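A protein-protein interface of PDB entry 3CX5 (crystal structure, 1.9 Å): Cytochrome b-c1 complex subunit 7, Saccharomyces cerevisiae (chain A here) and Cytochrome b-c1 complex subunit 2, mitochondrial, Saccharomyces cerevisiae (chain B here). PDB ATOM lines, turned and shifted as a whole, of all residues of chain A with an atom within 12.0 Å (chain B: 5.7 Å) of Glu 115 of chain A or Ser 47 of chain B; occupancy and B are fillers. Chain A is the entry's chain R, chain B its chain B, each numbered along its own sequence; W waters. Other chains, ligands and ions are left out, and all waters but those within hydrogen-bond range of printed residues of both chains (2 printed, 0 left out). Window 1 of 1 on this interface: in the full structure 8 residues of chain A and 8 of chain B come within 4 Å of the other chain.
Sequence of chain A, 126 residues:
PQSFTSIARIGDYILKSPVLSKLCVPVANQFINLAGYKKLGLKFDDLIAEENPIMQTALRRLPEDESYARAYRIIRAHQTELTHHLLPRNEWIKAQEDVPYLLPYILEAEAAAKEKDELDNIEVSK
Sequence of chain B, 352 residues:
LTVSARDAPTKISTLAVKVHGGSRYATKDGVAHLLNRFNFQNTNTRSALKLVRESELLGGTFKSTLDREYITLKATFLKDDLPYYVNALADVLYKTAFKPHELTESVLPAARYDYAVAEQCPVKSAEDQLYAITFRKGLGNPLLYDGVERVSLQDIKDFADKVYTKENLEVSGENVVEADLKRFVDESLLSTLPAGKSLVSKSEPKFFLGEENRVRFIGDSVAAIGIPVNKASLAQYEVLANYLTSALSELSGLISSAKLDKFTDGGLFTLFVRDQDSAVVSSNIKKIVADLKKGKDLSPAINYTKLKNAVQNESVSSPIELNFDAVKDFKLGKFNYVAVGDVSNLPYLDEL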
ATOM      1  N   SER A   3     -27.618  -1.142   6.651  1.00  0.00           N
ATOM      2  CA  SER A   3     -28.204   0.071   7.212  1.00  0.00           C
ATOM      3  C   SER A   3     -28.013   1.252   6.269  1.00  0.00           C
ATOM      4  O   SER A   3     -27.097   1.256   5.445  1.00  0.00           O
ATOM      5  CB  SER A   3     -27.568   0.396   8.563  1.00  0.00           C
ATOM      6  OG  SER A   3     -26.244   0.885   8.392  1.00  0.00           O
ATOM      7  N   THR A   5     -27.230   4.159   7.257  1.00  0.00           N
ATOM      8  CA  THR A   5     -26.104   4.915   7.791  1.00  0.00           C
ATOM      9  C   THR A   5     -24.857   4.435   7.057  1.00  0.00           C
ATOM     10  O   THR A   5     -23.963   5.223   6.749  1.00  0.00           O
ATOM     11  CB  THR A   5     -25.925   4.671   9.309  1.00  0.00           C
ATOM     12  OG1 THR A   5     -27.094   5.120  10.004  1.00  0.00           O
ATOM     13  CG2 THR A   5     -24.713   5.436   9.845  1.00  0.00           C
ATOM     14  N   ILE A  54     -37.419   0.475  12.174  1.00  0.00           N
ATOM     15  CA  ILE A  54     -36.806   1.724  11.725  1.00  0.00           C
ATOM     16  C   ILE A  54     -37.717   2.437  10.726  1.00  0.00           C
ATOM     17  O   ILE A  54     -38.031   3.612  10.887  1.00  0.00           O
ATOM     18  CB  ILE A  54     -35.417   1.491  11.068  1.00  0.00           C
ATOM     19  CG1 ILE A  54     -34.401   0.989  12.107  1.00  0.00           C
ATOM     20  CG2 ILE A  54     -34.912   2.776  10.400  1.00  0.00           C
ATOM     21  CD1 ILE A  54     -34.127   1.958  13.235  1.00  0.00           C
ATOM     22  N   ARG A  61     -43.294   9.466  11.423  1.00  0.00           N
ATOM     23  CA  ARG A  61     -42.806  10.834  11.570  1.00  0.00           C
ATOM     24  C   ARG A  61     -42.893  11.682  10.294  1.00  0.00           C
ATOM     25  O   ARG A  61     -42.732  12.905  10.337  1.00  0.00           O
ATOM     26  CB  ARG A  61     -41.376  10.822  12.124  1.00  0.00           C
ATOM     27  CG  ARG A  61     -41.333  11.001  13.621  1.00  0.00           C
ATOM     28  CD  ARG A  61     -40.787   9.823  14.402  1.00  0.00           C
ATOM     29  NE  ARG A  61     -39.332   9.797  14.466  1.00  0.00           N
ATOM     30  CZ  ARG A  61     -38.619   9.440  15.538  1.00  0.00           C
ATOM     31  NH1 ARG A  61     -37.296   9.428  15.470  1.00  0.00           N
ATOM     32  NH2 ARG A  61     -39.207   9.147  16.688  1.00  0.00           N
ATOM     33  N   ILE A 106     -35.138   8.257   8.360  1.00  0.00           N
ATOM     34  CA  ILE A 106     -34.543   6.937   8.544  1.00  0.00           C
ATOM     35  C   ILE A 106     -33.210   7.025   9.304  1.00  0.00           C
ATOM     36  O   ILE A 106     -32.977   6.270  10.256  1.00  0.00           O
ATOM     37  CB  ILE A 106     -34.295   6.237   7.185  1.00  0.00           C
ATOM     38  CG1 ILE A 106     -35.626   6.018   6.451  1.00  0.00           C
ATOM     39  CG2 ILE A 106     -33.585   4.909   7.400  1.00  0.00           C
ATOM     40  CD1 ILE A 106     -35.471   5.517   5.026  1.00  0.00           C
ATOM     41  N   LEU A 107     -32.340   7.941   8.877  1.00  0.00           N
ATOM     42  CA  LEU A 107     -31.028   8.112   9.510  1.00  0.00           C
ATOM     43  C   LEU A 107     -31.135   8.494  10.977  1.00  0.00           C
ATOM     44  O   LEU A 107     -30.366   8.015  11.812  1.00  0.00           O
ATOM     45  CB  LEU A 107     -30.195   9.152   8.751  1.00  0.00           C
ATOM     46  CG  LEU A 107     -29.747   8.728   7.345  1.00  0.00           C
ATOM     47  CD1 LEU A 107     -29.119   9.909   6.606  1.00  0.00           C
ATOM     48  CD2 LEU A 107     -28.766   7.571   7.448  1.00  0.00           C
ATOM     49  N   GLU A 108     -32.105   9.343  11.287  1.00  0.00           N
ATOM     50  CA  GLU A 108     -32.346   9.796  12.652  1.00  0.00           C
ATOM     51  C   GLU A 108     -32.807   8.624  13.521  1.00  0.00           C
ATOM     52  O   GLU A 108     -32.320   8.439  14.642  1.00  0.00           O
ATOM     53  CB  GLU A 108     -33.401  10.897  12.638  1.00  0.00           C
ATOM     54  CG  GLU A 108     -33.847  11.374  14.003  1.00  0.00           C
ATOM     55  CD  GLU A 108     -34.819  12.538  13.905  1.00  0.00           C
ATOM     56  OE1 GLU A 108     -34.550  13.580  14.537  1.00  0.00           O
ATOM     57  OE2 GLU A 108     -35.846  12.417  13.192  1.00  0.00           O
ATOM     58  N   ALA A 109     -33.730   7.824  12.989  1.00  0.00           N
ATOM     59  CA  ALA A 109     -34.237   6.658  13.707  1.00  0.00           C
ATOM     60  C   ALA A 109     -33.118   5.637  13.941  1.00  0.00           C
ATOM     61  O   ALA A 109     -33.028   5.054  15.020  1.00  0.00           O
ATOM     62  CB  ALA A 109     -35.402   6.013  12.938  1.00  0.00           C
ATOM     63  N   GLU A 110     -32.271   5.429  12.932  1.00  0.00           N
ATOM     64  CA  GLU A 110     -31.154   4.487  13.043  1.00  0.00           C
ATOM     65  C   GLU A 110     -30.132   4.934  14.088  1.00  0.00           C
ATOM     66  O   GLU A 110     -29.613   4.111  14.841  1.00  0.00           O
ATOM     67  CB  GLU A 110     -30.433   4.311  11.699  1.00  0.00           C
ATOM     68  CG  GLU A 110     -31.206   3.518  10.649  1.00  0.00           C
ATOM     69  CD  GLU A 110     -30.366   3.178   9.424  1.00  0.00           C
ATOM     70  OE1 GLU A 110     -30.848   2.407   8.567  1.00  0.00           O
ATOM     71  OE2 GLU A 110     -29.224   3.671   9.314  1.00  0.00           O
ATOM     72  N   ALA A 111     -29.823   6.229  14.098  1.00  0.00           N
ATOM     73  CA  ALA A 111     -28.866   6.786  15.048  1.00  0.00           C
ATOM     74  C   ALA A 111     -29.382   6.599  16.476  1.00  0.00           C
ATOM     75  O   ALA A 111     -28.625   6.210  17.361  1.00  0.00           O
ATOM     76  CB  ALA A 111     -28.605   8.274  14.744  1.00  0.00           C
ATOM     77  N   ALA A 112     -30.681   6.813  16.679  1.00  0.00           N
ATOM     78  CA  ALA A 112     -31.296   6.655  18.003  1.00  0.00           C
ATOM     79  C   ALA A 112     -31.293   5.190  18.446  1.00  0.00           C
ATOM     80  O   ALA A 112     -31.006   4.879  19.608  1.00  0.00           O
ATOM     81  CB  ALA A 112     -32.728   7.212  18.002  1.00  0.00           C
ATOM     82  N   ALA A 113     -31.592   4.289  17.513  1.00  0.00           N
ATOM     83  CA  ALA A 113     -31.608   2.861  17.818  1.00  0.00           C
ATOM     84  C   ALA A 113     -30.192   2.373  18.123  1.00  0.00           C
ATOM     85  O   ALA A 113     -29.992   1.573  19.035  1.00  0.00           O
ATOM     86  CB  ALA A 113     -32.215   2.070  16.660  1.00  0.00           C
ATOM     87  N   LYS A 114     -29.211   2.871  17.375  1.00  0.00           N
ATOM     88  CA  LYS A 114     -27.820   2.478  17.591  1.00  0.00           C
ATOM     89  C   LYS A 114     -27.364   2.900  18.992  1.00  0.00           C
ATOM     90  O   LYS A 114     -26.734   2.119  19.708  1.00  0.00           O
ATOM     91  CB  LYS A 114     -26.908   3.089  16.519  1.00  0.00           C
ATOM     92  CG  LYS A 114     -25.422   2.733  16.660  1.00  0.00           C
ATOM     93  CD  LYS A 114     -25.192   1.217  16.697  1.00  0.00           C
ATOM     94  CE  LYS A 114     -25.462   0.537  15.348  1.00  0.00           C
ATOM     95  NZ  LYS A 114     -24.417   0.855  14.328  1.00  0.00           N
ATOM     96  N   GLU A 115     -27.709   4.123  19.383  1.00  0.00           N
ATOM     97  CA  GLU A 115     -27.351   4.624  20.703  1.00  0.00           C
ATOM     98  C   GLU A 115     -28.042   3.829  21.815  1.00  0.00           C
ATOM     99  O   GLU A 115     -27.427   3.548  22.846  1.00  0.00           O
ATOM    100  CB  GLU A 115     -27.689   6.110  20.832  1.00  0.00           C
ATOM    101  CG  GLU A 115     -27.489   6.653  22.241  1.00  0.00           C
ATOM    102  CD  GLU A 115     -27.785   8.135  22.353  1.00  0.00           C
ATOM    103  OE1 GLU A 115     -28.964   8.526  22.234  1.00  0.00           O
ATOM    104  OE2 GLU A 115     -26.833   8.915  22.563  1.00  0.00           O
ATOM    105  N   LYS A 116     -29.311   3.468  21.615  1.00  0.00           N
ATOM    106  CA  LYS A 116     -30.034   2.695  22.625  1.00  0.00           C
ATOM    107  C   LYS A 116     -29.334   1.360  22.839  1.00  0.00           C
ATOM    108  O   LYS A 116     -29.123   0.944  23.974  1.00  0.00           O
ATOM    109  CB  LYS A 116     -31.499   2.457  22.230  1.00  0.00           C
ATOM    110  CG  LYS A 116     -32.315   1.823  23.361  1.00  0.00           C
ATOM    111  CD  LYS A 116     -33.763   1.559  22.978  1.00  0.00           C
ATOM    112  CE  LYS A 116     -34.587   1.138  24.194  1.00  0.00           C
ATOM    113  NZ  LYS A 116     -34.039  -0.060  24.903  1.00  0.00           N
ATOM    114  N   ASP A 117     -28.945   0.712  21.745  1.00  0.00           N
ATOM    115  CA  ASP A 117     -28.245  -0.568  21.811  1.00  0.00           C
ATOM    116  C   ASP A 117     -26.914  -0.407  22.557  1.00  0.00           C
ATOM    117  O   ASP A 117     -26.568  -1.232  23.410  1.00  0.00           O
ATOM    118  CB  ASP A 117     -28.000  -1.109  20.398  1.00  0.00           C
ATOM    119  CG  ASP A 117     -27.315  -2.467  20.399  1.00  0.00           C
ATOM    120  OD1 ASP A 117     -27.989  -3.476  20.708  1.00  0.00           O
ATOM    121  OD2 ASP A 117     -26.102  -2.525  20.090  1.00  0.00           O
ATOM    122  N   GLU A 118     -26.184   0.664  22.251  1.00  0.00           N
ATOM    123  CA  GLU A 118     -24.902   0.926  22.909  1.00  0.00           C
ATOM    124  C   GLU A 118     -25.111   1.132  24.407  1.00  0.00           C
ATOM    125  O   GLU A 118     -24.436   0.502  25.215  1.00  0.00           O
ATOM    126  CB  GLU A 118     -24.201   2.141  22.289  1.00  0.00           C
ATOM    127  CG  GLU A 118     -23.678   1.889  20.871  1.00  0.00           C
ATOM    128  CD  GLU A 118     -23.174   3.149  20.163  1.00  0.00           C
ATOM    129  OE1 GLU A 118     -23.571   4.275  20.542  1.00  0.00           O
ATOM    130  OE2 GLU A 118     -22.389   3.008  19.198  1.00  0.00           O
ATOM    131  N   LEU A 119     -26.093   1.958  24.767  1.00  0.00           N
ATOM    132  CA  LEU A 119     -26.387   2.233  26.174  1.00  0.00           C
ATOM    133  C   LEU A 119     -26.905   0.997  26.914  1.00  0.00           C
ATOM    134  O   LEU A 119     -26.618   0.816  28.099  1.00  0.00           O
ATOM    135  CB  LEU A 119     -27.366   3.411  26.310  1.00  0.00           C
ATOM    136  CG  LEU A 119     -26.802   4.771  25.875  1.00  0.00           C
ATOM    137  CD1 LEU A 119     -27.897   5.832  25.856  1.00  0.00           C
ATOM    138  CD2 LEU A 119     -25.665   5.187  26.809  1.00  0.00           C
ATOM    139  N   ASP A 120     -27.634   0.135  26.207  1.00  0.00           N
ATOM    140  CA  ASP A 120     -28.154  -1.097  26.801  1.00  0.00           C
ATOM    141  C   ASP A 120     -27.031  -2.077  27.125  1.00  0.00           C
ATOM    142  O   ASP A 120     -27.174  -2.908  28.021  1.00  0.00           O
ATOM    143  CB  ASP A 120     -29.149  -1.789  25.853  1.00  0.00           C
ATOM    144  CG  ASP A 120     -30.497  -1.087  25.794  1.00  0.00           C
ATOM    145  OD1 ASP A 120     -30.781  -0.247  26.671  1.00  0.00           O
ATOM    146  OD2 ASP A 120     -31.285  -1.389  24.870  1.00  0.00           O
ATOM    147  N   ASN A 121     -25.913  -1.963  26.410  1.00  0.00           N
ATOM    148  CA  ASN A 121     -24.781  -2.865  26.602  1.00  0.00           C
ATOM    149  C   ASN A 121     -23.488  -2.215  27.108  1.00  0.00           C
ATOM    150  O   ASN A 121     -22.416  -2.815  27.004  1.00  0.00           O
ATOM    151  CB  ASN A 121     -24.493  -3.611  25.291  1.00  0.00           C
ATOM    152  CG  ASN A 121     -25.630  -4.532  24.880  1.00  0.00           C
ATOM    153  OD1 ASN A 121     -25.872  -5.556  25.516  1.00  0.00           O
ATOM    154  ND2 ASN A 121     -26.343  -4.161  23.822  1.00  0.00           N
ATOM    155  N   ILE A 122     -23.583  -1.015  27.674  1.00  0.00           N
ATOM    156  CA  ILE A 122     -22.393  -0.320  28.165  1.00  0.00           C
ATOM    157  C   ILE A 122     -21.661  -1.087  29.252  1.00  0.00           C
ATOM    158  O   ILE A 122     -22.281  -1.754  30.074  1.00  0.00           O
ATOM    159  CB  ILE A 122     -22.710   1.088  28.706  1.00  0.00           C
ATOM    160  CG1 ILE A 122     -23.785   1.014  29.789  1.00  0.00           C
ATOM    161  CG2 ILE A 122     -23.081   2.018  27.569  1.00  0.00           C
ATOM    162  CD1 ILE A 122     -24.213   2.356  30.324  1.00  0.00           C
ATOM    163  N   GLU A 123     -20.336  -1.021  29.216  1.00  0.00           N
ATOM    164  CA  GLU A 123     -19.506  -1.688  30.208  1.00  0.00           C
ATOM    165  C   GLU A 123     -18.944  -0.628  31.147  1.00  0.00           C
ATOM    166  O   GLU A 123     -18.650   0.490  30.724  1.00  0.00           O
ATOM    167  CB  GLU A 123     -18.362  -2.454  29.533  1.00  0.00           C
ATOM    168  CG  GLU A 123     -18.826  -3.573  28.604  1.00  0.00           C
ATOM    169  CD  GLU A 123     -17.677  -4.349  27.962  1.00  0.00           C
ATOM    170  OE1 GLU A 123     -16.608  -3.752  27.699  1.00  0.00           O
ATOM    171  OE2 GLU A 123     -17.854  -5.561  27.705  1.00  0.00           O
ATOM    172  N   GLN B  41     -35.983  16.905  27.287  1.00  0.00           N
ATOM    173  CA  GLN B  41     -36.154  16.114  26.078  1.00  0.00           C
ATOM    174  C   GLN B  41     -34.777  16.255  25.401  1.00  0.00           C
ATOM    175  O   GLN B  41     -33.840  16.777  26.013  1.00  0.00           O
ATOM    176  CB  GLN B  41     -37.265  16.694  25.191  1.00  0.00           C
ATOM    177  CG  GLN B  41     -38.696  16.359  25.646  1.00  0.00           C
ATOM    178  CD  GLN B  41     -39.048  14.867  25.524  1.00  0.00           C
ATOM    179  OE1 GLN B  41     -39.787  14.331  26.344  1.00  0.00           O
ATOM    180  NE2 GLN B  41     -38.526  14.204  24.495  1.00  0.00           N
ATOM    181  N   ASN B  42     -34.636  15.803  24.160  1.00  0.00           N
ATOM    182  CA  ASN B  42     -33.353  15.905  23.459  1.00  0.00           C
ATOM    183  C   ASN B  42     -32.766  17.319  23.357  1.00  0.00           C
ATOM    184  O   ASN B  42     -33.496  18.301  23.219  1.00  0.00           O
ATOM    185  CB  ASN B  42     -33.471  15.379  22.022  1.00  0.00           C
ATOM    186  CG  ASN B  42     -33.741  13.888  21.949  1.00  0.00           C
ATOM    187  OD1 ASN B  42     -33.697  13.175  22.949  1.00  0.00           O
ATOM    188  ND2 ASN B  42     -34.025  13.412  20.745  1.00  0.00           N
ATOM    189  N   THR B  43     -31.444  17.409  23.484  1.00  0.00           N
ATOM    190  CA  THR B  43     -30.734  18.673  23.291  1.00  0.00           C
ATOM    191  C   THR B  43     -29.976  18.412  21.983  1.00  0.00           C
ATOM    192  O   THR B  43     -29.956  17.274  21.500  1.00  0.00           O
ATOM    193  CB  THR B  43     -29.728  19.021  24.430  1.00  0.00           C
ATOM    194  OG1 THR B  43     -28.636  18.096  24.427  1.00  0.00           O
ATOM    195  CG2 THR B  43     -30.414  19.010  25.794  1.00  0.00           C
ATOM    196  N   THR B  45     -26.860  18.207  21.447  1.00  0.00           N
ATOM    197  CA  THR B  45     -25.678  17.373  21.621  1.00  0.00           C
ATOM    198  C   THR B  45     -25.901  16.114  22.460  1.00  0.00           C
ATOM    199  O   THR B  45     -25.045  15.228  22.498  1.00  0.00           O
ATOM    200  CB  THR B  45     -24.523  18.193  22.229  1.00  0.00           C
ATOM    201  OG1 THR B  45     -24.942  18.744  23.482  1.00  0.00           O
ATOM    202  CG2 THR B  45     -24.122  19.333  21.293  1.00  0.00           C
ATOM    203  N   ARG B  46     -27.048  16.023  23.124  1.00  0.00           N
ATOM    204  CA  ARG B  46     -27.336  14.864  23.960  1.00  0.00           C
ATOM    205  C   ARG B  46     -28.831  14.524  23.998  1.00  0.00           C
ATOM    206  O   ARG B  46     -29.670  15.379  24.279  1.00  0.00           O
ATOM    207  CB  ARG B  46     -26.770  15.093  25.368  1.00  0.00           C
ATOM    208  CG  ARG B  46     -27.222  14.101  26.409  1.00  0.00           C
ATOM    209  CD  ARG B  46     -26.089  13.659  27.326  1.00  0.00           C
ATOM    210  NE  ARG B  46     -25.419  14.724  28.078  1.00  0.00           N
ATOM    211  CZ  ARG B  46     -26.025  15.703  28.750  1.00  0.00           C
ATOM    212  NH1 ARG B  46     -25.298  16.588  29.413  1.00  0.00           N
ATOM    213  NH2 ARG B  46     -27.343  15.842  28.711  1.00  0.00           N
ATOM    214  N   SER B  47     -29.149  13.277  23.666  1.00  0.00           N
ATOM    215  CA  SER B  47     -30.529  12.805  23.651  1.00  0.00           C
ATOM    216  C   SER B  47     -31.055  12.658  25.070  1.00  0.00           C
ATOM    217  O   SER B  47     -30.275  12.524  26.022  1.00  0.00           O
ATOM    218  CB  SER B  47     -30.624  11.445  22.943  1.00  0.00           C
ATOM    219  OG  SER B  47     -30.042  10.414  23.731  1.00  0.00           O
ATOM    220  N   ALA B  48     -32.379  12.658  25.198  1.00  0.00           N
ATOM    221  CA  ALA B  48     -33.043  12.499  26.486  1.00  0.00           C
ATOM    222  C   ALA B  48     -32.653  11.151  27.096  1.00  0.00           C
ATOM    223  O   ALA B  48     -32.459  11.043  28.305  1.00  0.00           O
ATOM    224  CB  ALA B  48     -34.562  12.588  26.311  1.00  0.00           C
ATOM    225  N   LEU B  49     -32.518  10.135  26.244  1.00  0.00           N
ATOM    226  CA  LEU B  49     -32.146   8.799  26.682  1.00  0.00           C
ATOM    227  C   LEU B  49     -30.742   8.777  27.288  1.00  0.00           C
ATOM    228  O   LEU B  49     -30.531   8.194  28.354  1.00  0.00           O
ATOM    229  CB  LEU B  49     -32.226   7.810  25.513  1.00  0.00           C
ATOM    230  CG  LEU B  49     -31.757   6.380  25.800  1.00  0.00           C
ATOM    231  CD1 LEU B  49     -32.700   5.723  26.803  1.00  0.00           C
ATOM    232  CD2 LEU B  49     -31.699   5.571  24.515  1.00  0.00           C
ATOM    233  N   LYS B  50     -29.782   9.399  26.608  1.00  0.00           N
ATOM    234  CA  LYS B  50     -28.413   9.422  27.118  1.00  0.00           C
ATOM    235  C   LYS B  50     -28.335  10.160  28.444  1.00  0.00           C
ATOM    236  O   LYS B  50     -27.643   9.721  29.362  1.00  0.00           O
ATOM    237  CB  LYS B  50     -27.443  10.047  26.116  1.00  0.00           C
ATOM    238  CG  LYS B  50     -25.988   9.883  26.539  1.00  0.00           C
ATOM    239  CD  LYS B  50     -25.033  10.200  25.415  1.00  0.00           C
ATOM    240  CE  LYS B  50     -23.634   9.704  25.760  1.00  0.00           C
ATOM    241  NZ  LYS B  50     -22.718   9.801  24.592  1.00  0.00           N
ATOM    242  N   LEU B  51     -29.064  11.268  28.543  1.00  0.00           N
ATOM    243  CA  LEU B  51     -29.089  12.054  29.767  1.00  0.00           C
ATOM    244  C   LEU B  51     -29.576  11.191  30.933  1.00  0.00           C
ATOM    245  O   LEU B  51     -28.972  11.187  32.005  1.00  0.00           O
ATOM    246  CB  LEU B  51     -29.998  13.279  29.595  1.00  0.00           C
ATOM    247  CG  LEU B  51     -30.113  14.225  30.796  1.00  0.00           C
ATOM    248  CD1 LEU B  51     -28.737  14.775  31.174  1.00  0.00           C
ATOM    249  CD2 LEU B  51     -31.066  15.356  30.460  1.00  0.00           C
ATOM    250  N   VAL B  52     -30.652  10.437  30.706  1.00  0.00           N
ATOM    251  CA  VAL B  52     -31.199   9.578  31.747  1.00  0.00           C
ATOM    252  C   VAL B  52     -30.233   8.462  32.144  1.00  0.00           C
ATOM    253  O   VAL B  52     -29.965   8.276  33.323  1.00  0.00           O
ATOM    254  CB  VAL B  52     -32.575   8.973  31.338  1.00  0.00           C
ATOM    255  CG1 VAL B  52     -32.996   7.884  32.322  1.00  0.00           C
ATOM    256  CG2 VAL B  52     -33.646  10.069  31.303  1.00  0.00           C
HETATM  257  O   HOH W   1     -24.180   8.432  22.383  1.00  0.00           O
HETATM  258  O   HOH W   2     -26.983  11.627  22.752  1.00  0.00           O
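The side-chain hydroxyl (OG) of Ser 47 of chain B sits at hydrogen-bond distance from the side-chain carboxylate (OE1) of Glu 115 of chain A.
The side-chain amino group of Lys 116 of chain A lies within salt-bridge range of the side-chain carboxylate of Asp 120 of chain A.
N of Lys 50 of chain B sits at hydrogen-bond distance from OG of Ser 47 of chain B (3.1 Å).
OE2 of Glu 115 of chain A touches CD of Lys 50 of chain B, 3.6 Å away.
Leu 49 of chain B touches Lys 116 of chain A (CD2 to CA, 3.8 Å).
CD1 of Leu 119 of chain A touches CG of Leu 49 of chain B, at 3.9 Å.
CA of Lys 50 of chain B touches CD1 of Leu 119 of chain A, 3.8 Å away.
Of chain B, only Ser 47 (2.6 Å) and Lys 50 (3.6 Å) come within 4 Å of Glu 115 of chain A.
No residue of chain A comes within 4 Å of Asn 42 of chain B.
No residue of chain A comes within 4 Å of Thr 43 of chain B.
No residue of chain A comes within 4 Å of Ala 48 of chain B.
Leu 49 of chain B touches just these residues of chain A: Lys 116 and Leu 119.
Printed residues of chain A within 4 Å of Lys 50 of chain B: Glu 115 (3.6 Å) and Leu 119 (3.8 Å).
Of the printed residues of chain B, Leu 119 of chain A touches Leu 49 and Lys 50.
Printed residues of chain B within 4 Å of Lys 116 of chain A: Leu 49.
The nearest residue of chain B that does not touch Glu 115 of chain A is Leu 49 of chain B (4.6 Å).
Hydrophobic or aromatic side chains of chain A within 4 Å of the printed part of chain B: Leu 119.
Along chain A the printed residues that touch a printed residue of chain B span positions 115 to 119.
Printed residues of chain B that touch a printed residue of chain A: Ser 47, Leu 49 and Lys 50.
Among the printed residues, 5 pairs touch across the chains.
Among the printed residues, no Asp or Glu carboxylate lies within 4 Å of a Lys or Arg side-chain nitrogen of the other chain.
Water W1 bridges OE2 of Glu 115 of chain A (2.7 Å) and NZ of Lys 50 of chain B (3.0 Å).
Water W2 lies within hydrogen-bond range of OE2 of Glu 115 of chain A (2.7 Å) and N of Ser 47 of chain B (2.9 Å).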
